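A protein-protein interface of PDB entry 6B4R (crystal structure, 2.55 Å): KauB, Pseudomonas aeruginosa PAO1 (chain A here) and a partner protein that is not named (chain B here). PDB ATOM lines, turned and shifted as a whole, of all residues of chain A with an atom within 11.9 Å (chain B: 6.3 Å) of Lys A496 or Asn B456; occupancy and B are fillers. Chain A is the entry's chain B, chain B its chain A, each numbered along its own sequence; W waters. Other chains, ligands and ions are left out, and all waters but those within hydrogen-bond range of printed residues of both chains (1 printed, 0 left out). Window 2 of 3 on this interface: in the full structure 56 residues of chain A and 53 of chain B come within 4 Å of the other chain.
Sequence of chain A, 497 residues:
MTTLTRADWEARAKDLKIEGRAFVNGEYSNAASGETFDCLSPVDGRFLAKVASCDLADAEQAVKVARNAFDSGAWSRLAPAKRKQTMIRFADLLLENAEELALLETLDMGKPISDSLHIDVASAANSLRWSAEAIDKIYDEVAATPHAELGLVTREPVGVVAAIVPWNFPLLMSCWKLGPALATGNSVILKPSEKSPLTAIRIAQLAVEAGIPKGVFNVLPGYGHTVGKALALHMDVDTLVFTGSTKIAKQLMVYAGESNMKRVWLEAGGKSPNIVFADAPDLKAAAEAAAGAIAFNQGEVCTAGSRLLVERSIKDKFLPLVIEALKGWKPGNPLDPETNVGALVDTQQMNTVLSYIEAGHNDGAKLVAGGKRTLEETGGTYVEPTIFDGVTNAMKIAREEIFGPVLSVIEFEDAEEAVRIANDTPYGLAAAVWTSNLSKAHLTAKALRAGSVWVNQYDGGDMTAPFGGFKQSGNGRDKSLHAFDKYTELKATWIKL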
ATOM      1  N   THR A 145      -7.321   6.422  -0.791  1.00  0.00           N
ATOM      2  CA  THR A 145      -6.798   6.973  -2.032  1.00  0.00           C
ATOM      3  C   THR A 145      -6.555   5.850  -3.035  1.00  0.00           C
ATOM      4  O   THR A 145      -6.575   4.678  -2.665  1.00  0.00           O
ATOM      5  CB  THR A 145      -5.465   7.706  -1.773  1.00  0.00           C
ATOM      6  OG1 THR A 145      -4.490   6.774  -1.292  1.00  0.00           O
ATOM      7  CG2 THR A 145      -5.651   8.811  -0.745  1.00  0.00           C
ATOM      8  N   PRO A 146      -6.339   6.203  -4.316  1.00  0.00           N
ATOM      9  CA  PRO A 146      -5.879   5.205  -5.288  1.00  0.00           C
ATOM     10  C   PRO A 146      -4.609   4.499  -4.813  1.00  0.00           C
ATOM     11  O   PRO A 146      -3.874   5.044  -3.987  1.00  0.00           O
ATOM     12  CB  PRO A 146      -5.584   6.048  -6.528  1.00  0.00           C
ATOM     13  CG  PRO A 146      -6.558   7.171  -6.438  1.00  0.00           C
ATOM     14  CD  PRO A 146      -6.691   7.480  -4.968  1.00  0.00           C
ATOM     15  N   HIS A 147      -4.367   3.302  -5.338  1.00  0.00           N
ATOM     16  CA  HIS A 147      -3.280   2.444  -4.872  1.00  0.00           C
ATOM     17  C   HIS A 147      -1.902   3.096  -4.972  1.00  0.00           C
ATOM     18  O   HIS A 147      -1.058   2.918  -4.095  1.00  0.00           O
ATOM     19  CB  HIS A 147      -3.284   1.123  -5.646  1.00  0.00           C
ATOM     20  CG  HIS A 147      -2.398   0.073  -5.054  1.00  0.00           C
ATOM     21  ND1 HIS A 147      -2.739  -0.637  -3.923  1.00  0.00           N
ATOM     22  CD2 HIS A 147      -1.180  -0.384  -5.431  1.00  0.00           C
ATOM     23  CE1 HIS A 147      -1.773  -1.488  -3.632  1.00  0.00           C
ATOM     24  NE2 HIS A 147      -0.815  -1.355  -4.531  1.00  0.00           N
ATOM     25  N   ALA A 148      -1.680   3.854  -6.040  1.00  0.00           N
ATOM     26  CA  ALA A 148      -0.380   4.469  -6.282  1.00  0.00           C
ATOM     27  C   ALA A 148      -0.205   5.771  -5.504  1.00  0.00           C
ATOM     28  O   ALA A 148       0.645   6.594  -5.840  1.00  0.00           O
ATOM     29  CB  ALA A 148      -0.187   4.715  -7.771  1.00  0.00           C
ATOM     30  N   GLU A 149      -1.008   5.957  -4.463  1.00  0.00           N
ATOM     31  CA  GLU A 149      -0.966   7.193  -3.697  1.00  0.00           C
ATOM     32  C   GLU A 149      -1.080   6.937  -2.198  1.00  0.00           C
ATOM     33  O   GLU A 149      -1.770   6.015  -1.768  1.00  0.00           O
ATOM     34  CB  GLU A 149      -2.075   8.137  -4.163  1.00  0.00           C
ATOM     35  CG  GLU A 149      -1.640   9.590  -4.273  1.00  0.00           C
ATOM     36  CD  GLU A 149      -2.601  10.430  -5.095  1.00  0.00           C
ATOM     37  OE1 GLU A 149      -3.624   9.884  -5.566  1.00  0.00           O
ATOM     38  OE2 GLU A 149      -2.331  11.638  -5.270  1.00  0.00           O
ATOM     39  N   LEU A 150      -0.387   7.754  -1.411  1.00  0.00           N
ATOM     40  CA  LEU A 150      -0.485   7.696   0.042  1.00  0.00           C
ATOM     41  C   LEU A 150      -0.887   9.062   0.581  1.00  0.00           C
ATOM     42  O   LEU A 150      -0.173  10.047   0.389  1.00  0.00           O
ATOM     43  CB  LEU A 150       0.840   7.249   0.665  1.00  0.00           C
ATOM     44  CG  LEU A 150       0.887   7.222   2.196  1.00  0.00           C
ATOM     45  CD1 LEU A 150      -0.138   6.248   2.759  1.00  0.00           C
ATOM     46  CD2 LEU A 150       2.285   6.882   2.696  1.00  0.00           C
ATOM     47  N   GLY A 151      -2.034   9.116   1.251  1.00  0.00           N
ATOM     48  CA  GLY A 151      -2.575  10.372   1.739  1.00  0.00           C
ATOM     49  C   GLY A 151      -2.653  10.449   3.250  1.00  0.00           C
ATOM     50  O   GLY A 151      -3.515   9.821   3.869  1.00  0.00           O
ATOM     51  N   LEU A 152      -1.756  11.232   3.841  1.00  0.00           N
ATOM     52  CA  LEU A 152      -1.688  11.369   5.292  1.00  0.00           C
ATOM     53  C   LEU A 152      -2.389  12.636   5.769  1.00  0.00           C
ATOM     54  O   LEU A 152      -2.288  13.689   5.140  1.00  0.00           O
ATOM     55  CB  LEU A 152      -0.233  11.387   5.760  1.00  0.00           C
ATOM     56  CG  LEU A 152       0.672  10.278   5.224  1.00  0.00           C
ATOM     57  CD1 LEU A 152       2.067  10.403   5.813  1.00  0.00           C
ATOM     58  CD2 LEU A 152       0.073   8.914   5.524  1.00  0.00           C
ATOM     59  N   ALA A 492      -2.253  17.918   5.197  1.00  0.00           N
ATOM     60  CA  ALA A 492      -2.574  16.850   4.257  1.00  0.00           C
ATOM     61  C   ALA A 492      -1.385  16.578   3.343  1.00  0.00           C
ATOM     62  O   ALA A 492      -1.115  17.344   2.418  1.00  0.00           O
ATOM     63  CB  ALA A 492      -3.803  17.211   3.437  1.00  0.00           C
ATOM     64  N   THR A 493      -0.676  15.485   3.606  1.00  0.00           N
ATOM     65  CA  THR A 493       0.475  15.117   2.790  1.00  0.00           C
ATOM     66  C   THR A 493       0.110  14.040   1.772  1.00  0.00           C
ATOM     67  O   THR A 493      -0.059  12.875   2.126  1.00  0.00           O
ATOM     68  CB  THR A 493       1.644  14.620   3.657  1.00  0.00           C
ATOM     69  OG1 THR A 493       1.994  15.629   4.612  1.00  0.00           O
ATOM     70  CG2 THR A 493       2.853  14.305   2.791  1.00  0.00           C
ATOM     71  N   TRP A 494      -0.012  14.440   0.508  1.00  0.00           N
ATOM     72  CA  TRP A 494      -0.362  13.512  -0.564  1.00  0.00           C
ATOM     73  C   TRP A 494       0.861  13.089  -1.373  1.00  0.00           C
ATOM     74  O   TRP A 494       1.458  13.895  -2.085  1.00  0.00           O
ATOM     75  CB  TRP A 494      -1.436  14.112  -1.476  1.00  0.00           C
ATOM     76  CG  TRP A 494      -2.780  13.473  -1.296  1.00  0.00           C
ATOM     77  CD1 TRP A 494      -3.512  12.817  -2.245  1.00  0.00           C
ATOM     78  CD2 TRP A 494      -3.544  13.406  -0.086  1.00  0.00           C
ATOM     79  NE1 TRP A 494      -4.688  12.358  -1.703  1.00  0.00           N
ATOM     80  CE2 TRP A 494      -4.731  12.705  -0.379  1.00  0.00           C
ATOM     81  CE3 TRP A 494      -3.341  13.875   1.216  1.00  0.00           C
ATOM     82  CZ2 TRP A 494      -5.709  12.460   0.583  1.00  0.00           C
ATOM     83  CZ3 TRP A 494      -4.313  13.631   2.168  1.00  0.00           C
ATOM     84  CH2 TRP A 494      -5.482  12.928   1.847  1.00  0.00           C
ATOM     85  N   ILE A 495       1.216  11.813  -1.259  1.00  0.00           N
ATOM     86  CA  ILE A 495       2.439  11.288  -1.852  1.00  0.00           C
ATOM     87  C   ILE A 495       2.165  10.407  -3.068  1.00  0.00           C
ATOM     88  O   ILE A 495       1.508   9.370  -2.962  1.00  0.00           O
ATOM     89  CB  ILE A 495       3.235  10.474  -0.819  1.00  0.00           C
ATOM     90  CG1 ILE A 495       3.504  11.326   0.424  1.00  0.00           C
ATOM     91  CG2 ILE A 495       4.530   9.950  -1.427  1.00  0.00           C
ATOM     92  CD1 ILE A 495       4.071  10.550   1.589  1.00  0.00           C
ATOM     93  N   LYS A 496       2.677  10.827  -4.222  1.00  0.00           N
ATOM     94  CA  LYS A 496       2.547  10.048  -5.447  1.00  0.00           C
ATOM     95  C   LYS A 496       3.586   8.935  -5.488  1.00  0.00           C
ATOM     96  O   LYS A 496       4.790   9.197  -5.483  1.00  0.00           O
ATOM     97  CB  LYS A 496       2.702  10.942  -6.677  1.00  0.00           C
ATOM     98  CG  LYS A 496       2.673  10.178  -7.991  1.00  0.00           C
ATOM     99  CD  LYS A 496       1.294  10.211  -8.632  1.00  0.00           C
ATOM    100  CE  LYS A 496       1.016  11.566  -9.268  1.00  0.00           C
ATOM    101  NZ  LYS A 496      -0.276  11.592 -10.009  1.00  0.00           N
ATOM    102  N   LEU A 497       3.115   7.694  -5.530  1.00  0.00           N
ATOM    103  CA  LEU A 497       4.003   6.540  -5.580  1.00  0.00           C
ATOM    104  C   LEU A 497       4.201   6.074  -7.019  1.00  0.00           C
ATOM    105  O   LEU A 497       5.134   5.328  -7.316  1.00  0.00           O
ATOM    106  CB  LEU A 497       3.442   5.399  -4.727  1.00  0.00           C
ATOM    107  CG  LEU A 497       3.108   5.732  -3.270  1.00  0.00           C
ATOM    108  CD1 LEU A 497       2.409   4.556  -2.603  1.00  0.00           C
ATOM    109  CD2 LEU A 497       4.361   6.122  -2.498  1.00  0.00           C
ATOM    110  N   ALA B 280      15.113  13.799  -7.870  1.00  0.00           N
ATOM    111  CA  ALA B 280      13.712  13.660  -8.254  1.00  0.00           C
ATOM    112  C   ALA B 280      13.520  12.452  -9.174  1.00  0.00           C
ATOM    113  O   ALA B 280      14.359  12.187 -10.033  1.00  0.00           O
ATOM    114  CB  ALA B 280      13.222  14.931  -8.928  1.00  0.00           C
ATOM    115  N   PRO B 281      12.417  11.708  -8.987  1.00  0.00           N
ATOM    116  CA  PRO B 281      12.119  10.501  -9.770  1.00  0.00           C
ATOM    117  C   PRO B 281      12.129  10.757 -11.276  1.00  0.00           C
ATOM    118  O   PRO B 281      12.677   9.958 -12.034  1.00  0.00           O
ATOM    119  CB  PRO B 281      10.702  10.133  -9.316  1.00  0.00           C
ATOM    120  CG  PRO B 281      10.591  10.694  -7.948  1.00  0.00           C
ATOM    121  CD  PRO B 281      11.381  11.976  -7.975  1.00  0.00           C
ATOM    122  N   ALA B 432       5.340  21.778  -2.206  1.00  0.00           N
ATOM    123  CA  ALA B 432       5.620  20.532  -2.915  1.00  0.00           C
ATOM    124  C   ALA B 432       7.082  20.122  -2.801  1.00  0.00           C
ATOM    125  O   ALA B 432       7.970  20.968  -2.725  1.00  0.00           O
ATOM    126  CB  ALA B 432       5.211  20.636  -4.373  1.00  0.00           C
ATOM    127  N   VAL B 433       7.319  18.815  -2.776  1.00  0.00           N
ATOM    128  CA  VAL B 433       8.671  18.273  -2.718  1.00  0.00           C
ATOM    129  C   VAL B 433       8.847  17.162  -3.748  1.00  0.00           C
ATOM    130  O   VAL B 433       8.034  16.244  -3.828  1.00  0.00           O
ATOM    131  CB  VAL B 433       9.002  17.724  -1.315  1.00  0.00           C
ATOM    132  CG1 VAL B 433      10.344  17.010  -1.326  1.00  0.00           C
ATOM    133  CG2 VAL B 433       9.008  18.846  -0.294  1.00  0.00           C
ATOM    134  N   TRP B 434       9.908  17.259  -4.540  1.00  0.00           N
ATOM    135  CA  TRP B 434      10.218  16.240  -5.533  1.00  0.00           C
ATOM    136  C   TRP B 434      11.526  15.537  -5.192  1.00  0.00           C
ATOM    137  O   TRP B 434      12.603  16.128  -5.274  1.00  0.00           O
ATOM    138  CB  TRP B 434      10.280  16.858  -6.930  1.00  0.00           C
ATOM    139  CG  TRP B 434       8.972  17.454  -7.361  1.00  0.00           C
ATOM    140  CD1 TRP B 434       8.438  18.640  -6.952  1.00  0.00           C
ATOM    141  CD2 TRP B 434       8.031  16.886  -8.281  1.00  0.00           C
ATOM    142  NE1 TRP B 434       7.221  18.846  -7.558  1.00  0.00           N
ATOM    143  CE2 TRP B 434       6.950  17.785  -8.381  1.00  0.00           C
ATOM    144  CE3 TRP B 434       7.997  15.706  -9.030  1.00  0.00           C
ATOM    145  CZ2 TRP B 434       5.850  17.541  -9.199  1.00  0.00           C
ATOM    146  CZ3 TRP B 434       6.905  15.465  -9.840  1.00  0.00           C
ATOM    147  CH2 TRP B 434       5.846  16.379  -9.920  1.00  0.00           C
ATOM    148  N   THR B 435      11.418  14.273  -4.795  1.00  0.00           N
ATOM    149  CA  THR B 435      12.577  13.467  -4.437  1.00  0.00           C
ATOM    150  C   THR B 435      12.191  11.994  -4.442  1.00  0.00           C
ATOM    151  O   THR B 435      11.022  11.650  -4.275  1.00  0.00           O
ATOM    152  CB  THR B 435      13.135  13.852  -3.048  1.00  0.00           C
ATOM    153  OG1 THR B 435      14.252  13.015  -2.721  1.00  0.00           O
ATOM    154  CG2 THR B 435      12.072  13.695  -1.980  1.00  0.00           C
ATOM    155  N   SER B 436      13.178  11.127  -4.646  1.00  0.00           N
ATOM    156  CA  SER B 436      12.939   9.691  -4.663  1.00  0.00           C
ATOM    157  C   SER B 436      13.383   9.056  -3.352  1.00  0.00           C
ATOM    158  O   SER B 436      13.144   7.872  -3.112  1.00  0.00           O
ATOM    159  CB  SER B 436      13.674   9.041  -5.834  1.00  0.00           C
ATOM    160  OG  SER B 436      15.075   9.191  -5.699  1.00  0.00           O
ATOM    161  N   ALA B 441      11.992  12.720   1.707  1.00  0.00           N
ATOM    162  CA  ALA B 441      10.621  13.074   1.347  1.00  0.00           C
ATOM    163  C   ALA B 441       9.757  13.318   2.583  1.00  0.00           C
ATOM    164  O   ALA B 441       9.044  14.318   2.661  1.00  0.00           O
ATOM    165  CB  ALA B 441      10.000  11.993   0.469  1.00  0.00           C
ATOM    166  N   TRP B 454       2.527  18.276  -1.175  1.00  0.00           N
ATOM    167  CA  TRP B 454       2.461  17.296  -2.252  1.00  0.00           C
ATOM    168  C   TRP B 454       3.842  16.740  -2.580  1.00  0.00           C
ATOM    169  O   TRP B 454       4.797  17.490  -2.778  1.00  0.00           O
ATOM    170  CB  TRP B 454       1.790  17.900  -3.490  1.00  0.00           C
ATOM    171  CG  TRP B 454       0.410  18.418  -3.202  1.00  0.00           C
ATOM    172  CD1 TRP B 454      -0.628  17.719  -2.663  1.00  0.00           C
ATOM    173  CD2 TRP B 454      -0.079  19.746  -3.433  1.00  0.00           C
ATOM    174  NE1 TRP B 454      -1.734  18.527  -2.543  1.00  0.00           N
ATOM    175  CE2 TRP B 454      -1.423  19.776  -3.011  1.00  0.00           C
ATOM    176  CE3 TRP B 454       0.487  20.911  -3.960  1.00  0.00           C
ATOM    177  CZ2 TRP B 454      -2.208  20.924  -3.098  1.00  0.00           C
ATOM    178  CZ3 TRP B 454      -0.293  22.048  -4.046  1.00  0.00           C
ATOM    179  CH2 TRP B 454      -1.625  22.047  -3.616  1.00  0.00           C
ATOM    180  N   VAL B 455       3.943  15.416  -2.617  1.00  0.00           N
ATOM    181  CA  VAL B 455       5.216  14.754  -2.875  1.00  0.00           C
ATOM    182  C   VAL B 455       5.198  14.056  -4.228  1.00  0.00           C
ATOM    183  O   VAL B 455       4.325  13.228  -4.495  1.00  0.00           O
ATOM    184  CB  VAL B 455       5.553  13.724  -1.778  1.00  0.00           C
ATOM    185  CG1 VAL B 455       6.913  13.093  -2.043  1.00  0.00           C
ATOM    186  CG2 VAL B 455       5.523  14.378  -0.404  1.00  0.00           C
ATOM    187  N   ASN B 456       6.170  14.398  -5.072  1.00  0.00           N
ATOM    188  CA  ASN B 456       6.288  13.839  -6.420  1.00  0.00           C
ATOM    189  C   ASN B 456       5.034  14.042  -7.275  1.00  0.00           C
ATOM    190  O   ASN B 456       4.700  13.218  -8.127  1.00  0.00           O
ATOM    191  CB  ASN B 456       6.701  12.363  -6.368  1.00  0.00           C
ATOM    192  CG  ASN B 456       8.086  12.170  -5.779  1.00  0.00           C
ATOM    193  OD1 ASN B 456       8.925  13.067  -5.837  1.00  0.00           O
ATOM    194  ND2 ASN B 456       8.332  10.999  -5.205  1.00  0.00           N
ATOM    195  N   GLN B 457       4.352  15.155  -7.030  1.00  0.00           N
ATOM    196  CA  GLN B 457       3.180  15.562  -7.795  1.00  0.00           C
ATOM    197  C   GLN B 457       2.816  16.977  -7.373  1.00  0.00           C
ATOM    198  O   GLN B 457       3.318  17.478  -6.367  1.00  0.00           O
ATOM    199  CB  GLN B 457       2.001  14.630  -7.525  1.00  0.00           C
ATOM    200  CG  GLN B 457       1.532  14.634  -6.086  1.00  0.00           C
ATOM    201  CD  GLN B 457       0.264  13.826  -5.889  1.00  0.00           C
ATOM    202  OE1 GLN B 457      -0.657  13.880  -6.706  1.00  0.00           O
ATOM    203  NE2 GLN B 457       0.212  13.067  -4.801  1.00  0.00           N
ATOM    204  N   TYR B 458       1.948  17.626  -8.138  1.00  0.00           N
ATOM    205  CA  TYR B 458       1.453  18.930  -7.730  1.00  0.00           C
ATOM    206  C   TYR B 458      -0.069  18.984  -7.777  1.00  0.00           C
ATOM    207  O   TYR B 458      -0.697  18.289  -8.576  1.00  0.00           O
ATOM    208  CB  TYR B 458       2.064  20.055  -8.573  1.00  0.00           C
ATOM    209  CG  TYR B 458       2.074  21.374  -7.835  1.00  0.00           C
ATOM    210  CD1 TYR B 458       3.110  21.693  -6.965  1.00  0.00           C
ATOM    211  CD2 TYR B 458       1.037  22.285  -7.982  1.00  0.00           C
ATOM    212  CE1 TYR B 458       3.121  22.887  -6.272  1.00  0.00           C
ATOM    213  CE2 TYR B 458       1.039  23.485  -7.294  1.00  0.00           C
ATOM    214  CZ  TYR B 458       2.085  23.780  -6.440  1.00  0.00           C
ATOM    215  OH  TYR B 458       2.094  24.969  -5.749  1.00  0.00           O
HETATM  216  O   HOH W   1      -3.259  17.251  -0.033  1.00  0.00           O
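Of the 14 printed residues of chain A, 4 touch a printed residue of chain B. Hydrophobic or aromatic side chains of chain B within 4 Å of the printed part of chain A: Trp B454 and Val B455. Along chain B the printed residues that touch a printed residue of chain A span positions 454 to 457. Among the printed residues, no Asp or Glu carboxylate lies within 4 Å of a Lys or Arg side-chain nitrogen of the other chain.
Water W1 bridges the indole nitrogen of Trp B454 and the backbone carbonyl oxygen of Ala A492.
The backbone NH of Lys A496 sits at hydrogen-bond distance from the backbone carbonyl oxygen of Val B455, at 2.9 Å. The side-chain amide nitrogen of Gln B457 sits close to the backbone NH of Lys A496, 3.4 Å away. The backbone NH of Val B455 sits at hydrogen-bond distance from the backbone carbonyl oxygen of Trp A494, at 3.0 Å. NE2 of Gln B457 is in hydrogen-bond range of OE2 of Glu A149 (3.0 Å). The backbone carbonyl oxygen (O) of Trp A494 sits at hydrogen-bond distance from the side-chain amide nitrogen (NE2) of Gln B457 (3.1 Å).
Among the printed residues, pairs that only touch across the chains: Trp A494 with Trp B454 (3.5 Å), Ile A495 with Val B455 (3.8 Å), Ile A495 with Gln B457 (3.7 Å) and Lys A496 with Asn B456 (3.4 Å).
Lys A496 touches three residues of chain B. Asn B456 touches one residue of chain A. No residue of chain A comes within 4 Å of Ala B280. No residue of chain A comes within 4 Å of Trp B434. No residue of chain A comes within 4 Å of Ser B436. Val B455 touches just these residues of chain A: Trp A494 (3.0 Å), Ile A495 (3.8 Å) and Lys A496 (2.9 Å). Gln B457 touches just these residues of chain A: Glu A149 (3.0 Å), Trp A494 (3.1 Å), Ile A495 (3.7 Å) and Lys A496 (3.4 Å). Printed residues of chain B within 4 Å of Trp A494: Trp B454, Val B455 and Gln B457. Of the printed residues of chain A, Trp B454 touches Trp A494. Of the printed residues of chain B, Glu A149 touches Gln B457. Of the printed residues of chain B, Ile A495 touches Val B455 and Gln B457. The nearest printed residue of chain B that does not touch Lys A496 is Tyr B458 (6.2 Å). The nearest residue of chain A that does not touch Asn B456 is Ile A495 (5.5 Å).
N of Asn B456 sits at hydrogen-bond distance from O of Val B433 (2.9 Å). O of Leu A150 lies within hydrogen-bond range of N of Ile A495, at 2.8 Å. The backbone carbonyl oxygen (O) of Glu A149 sits at hydrogen-bond distance from the side-chain hydroxyl (OG1) of Thr A145 (2.9 Å). The backbone carbonyl oxygen of Thr B435 sits at hydrogen-bond distance from the side-chain amide nitrogen of Asn B456 (2.9 Å). N of Val B433 sits at hydrogen-bond distance from O of Trp B454.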
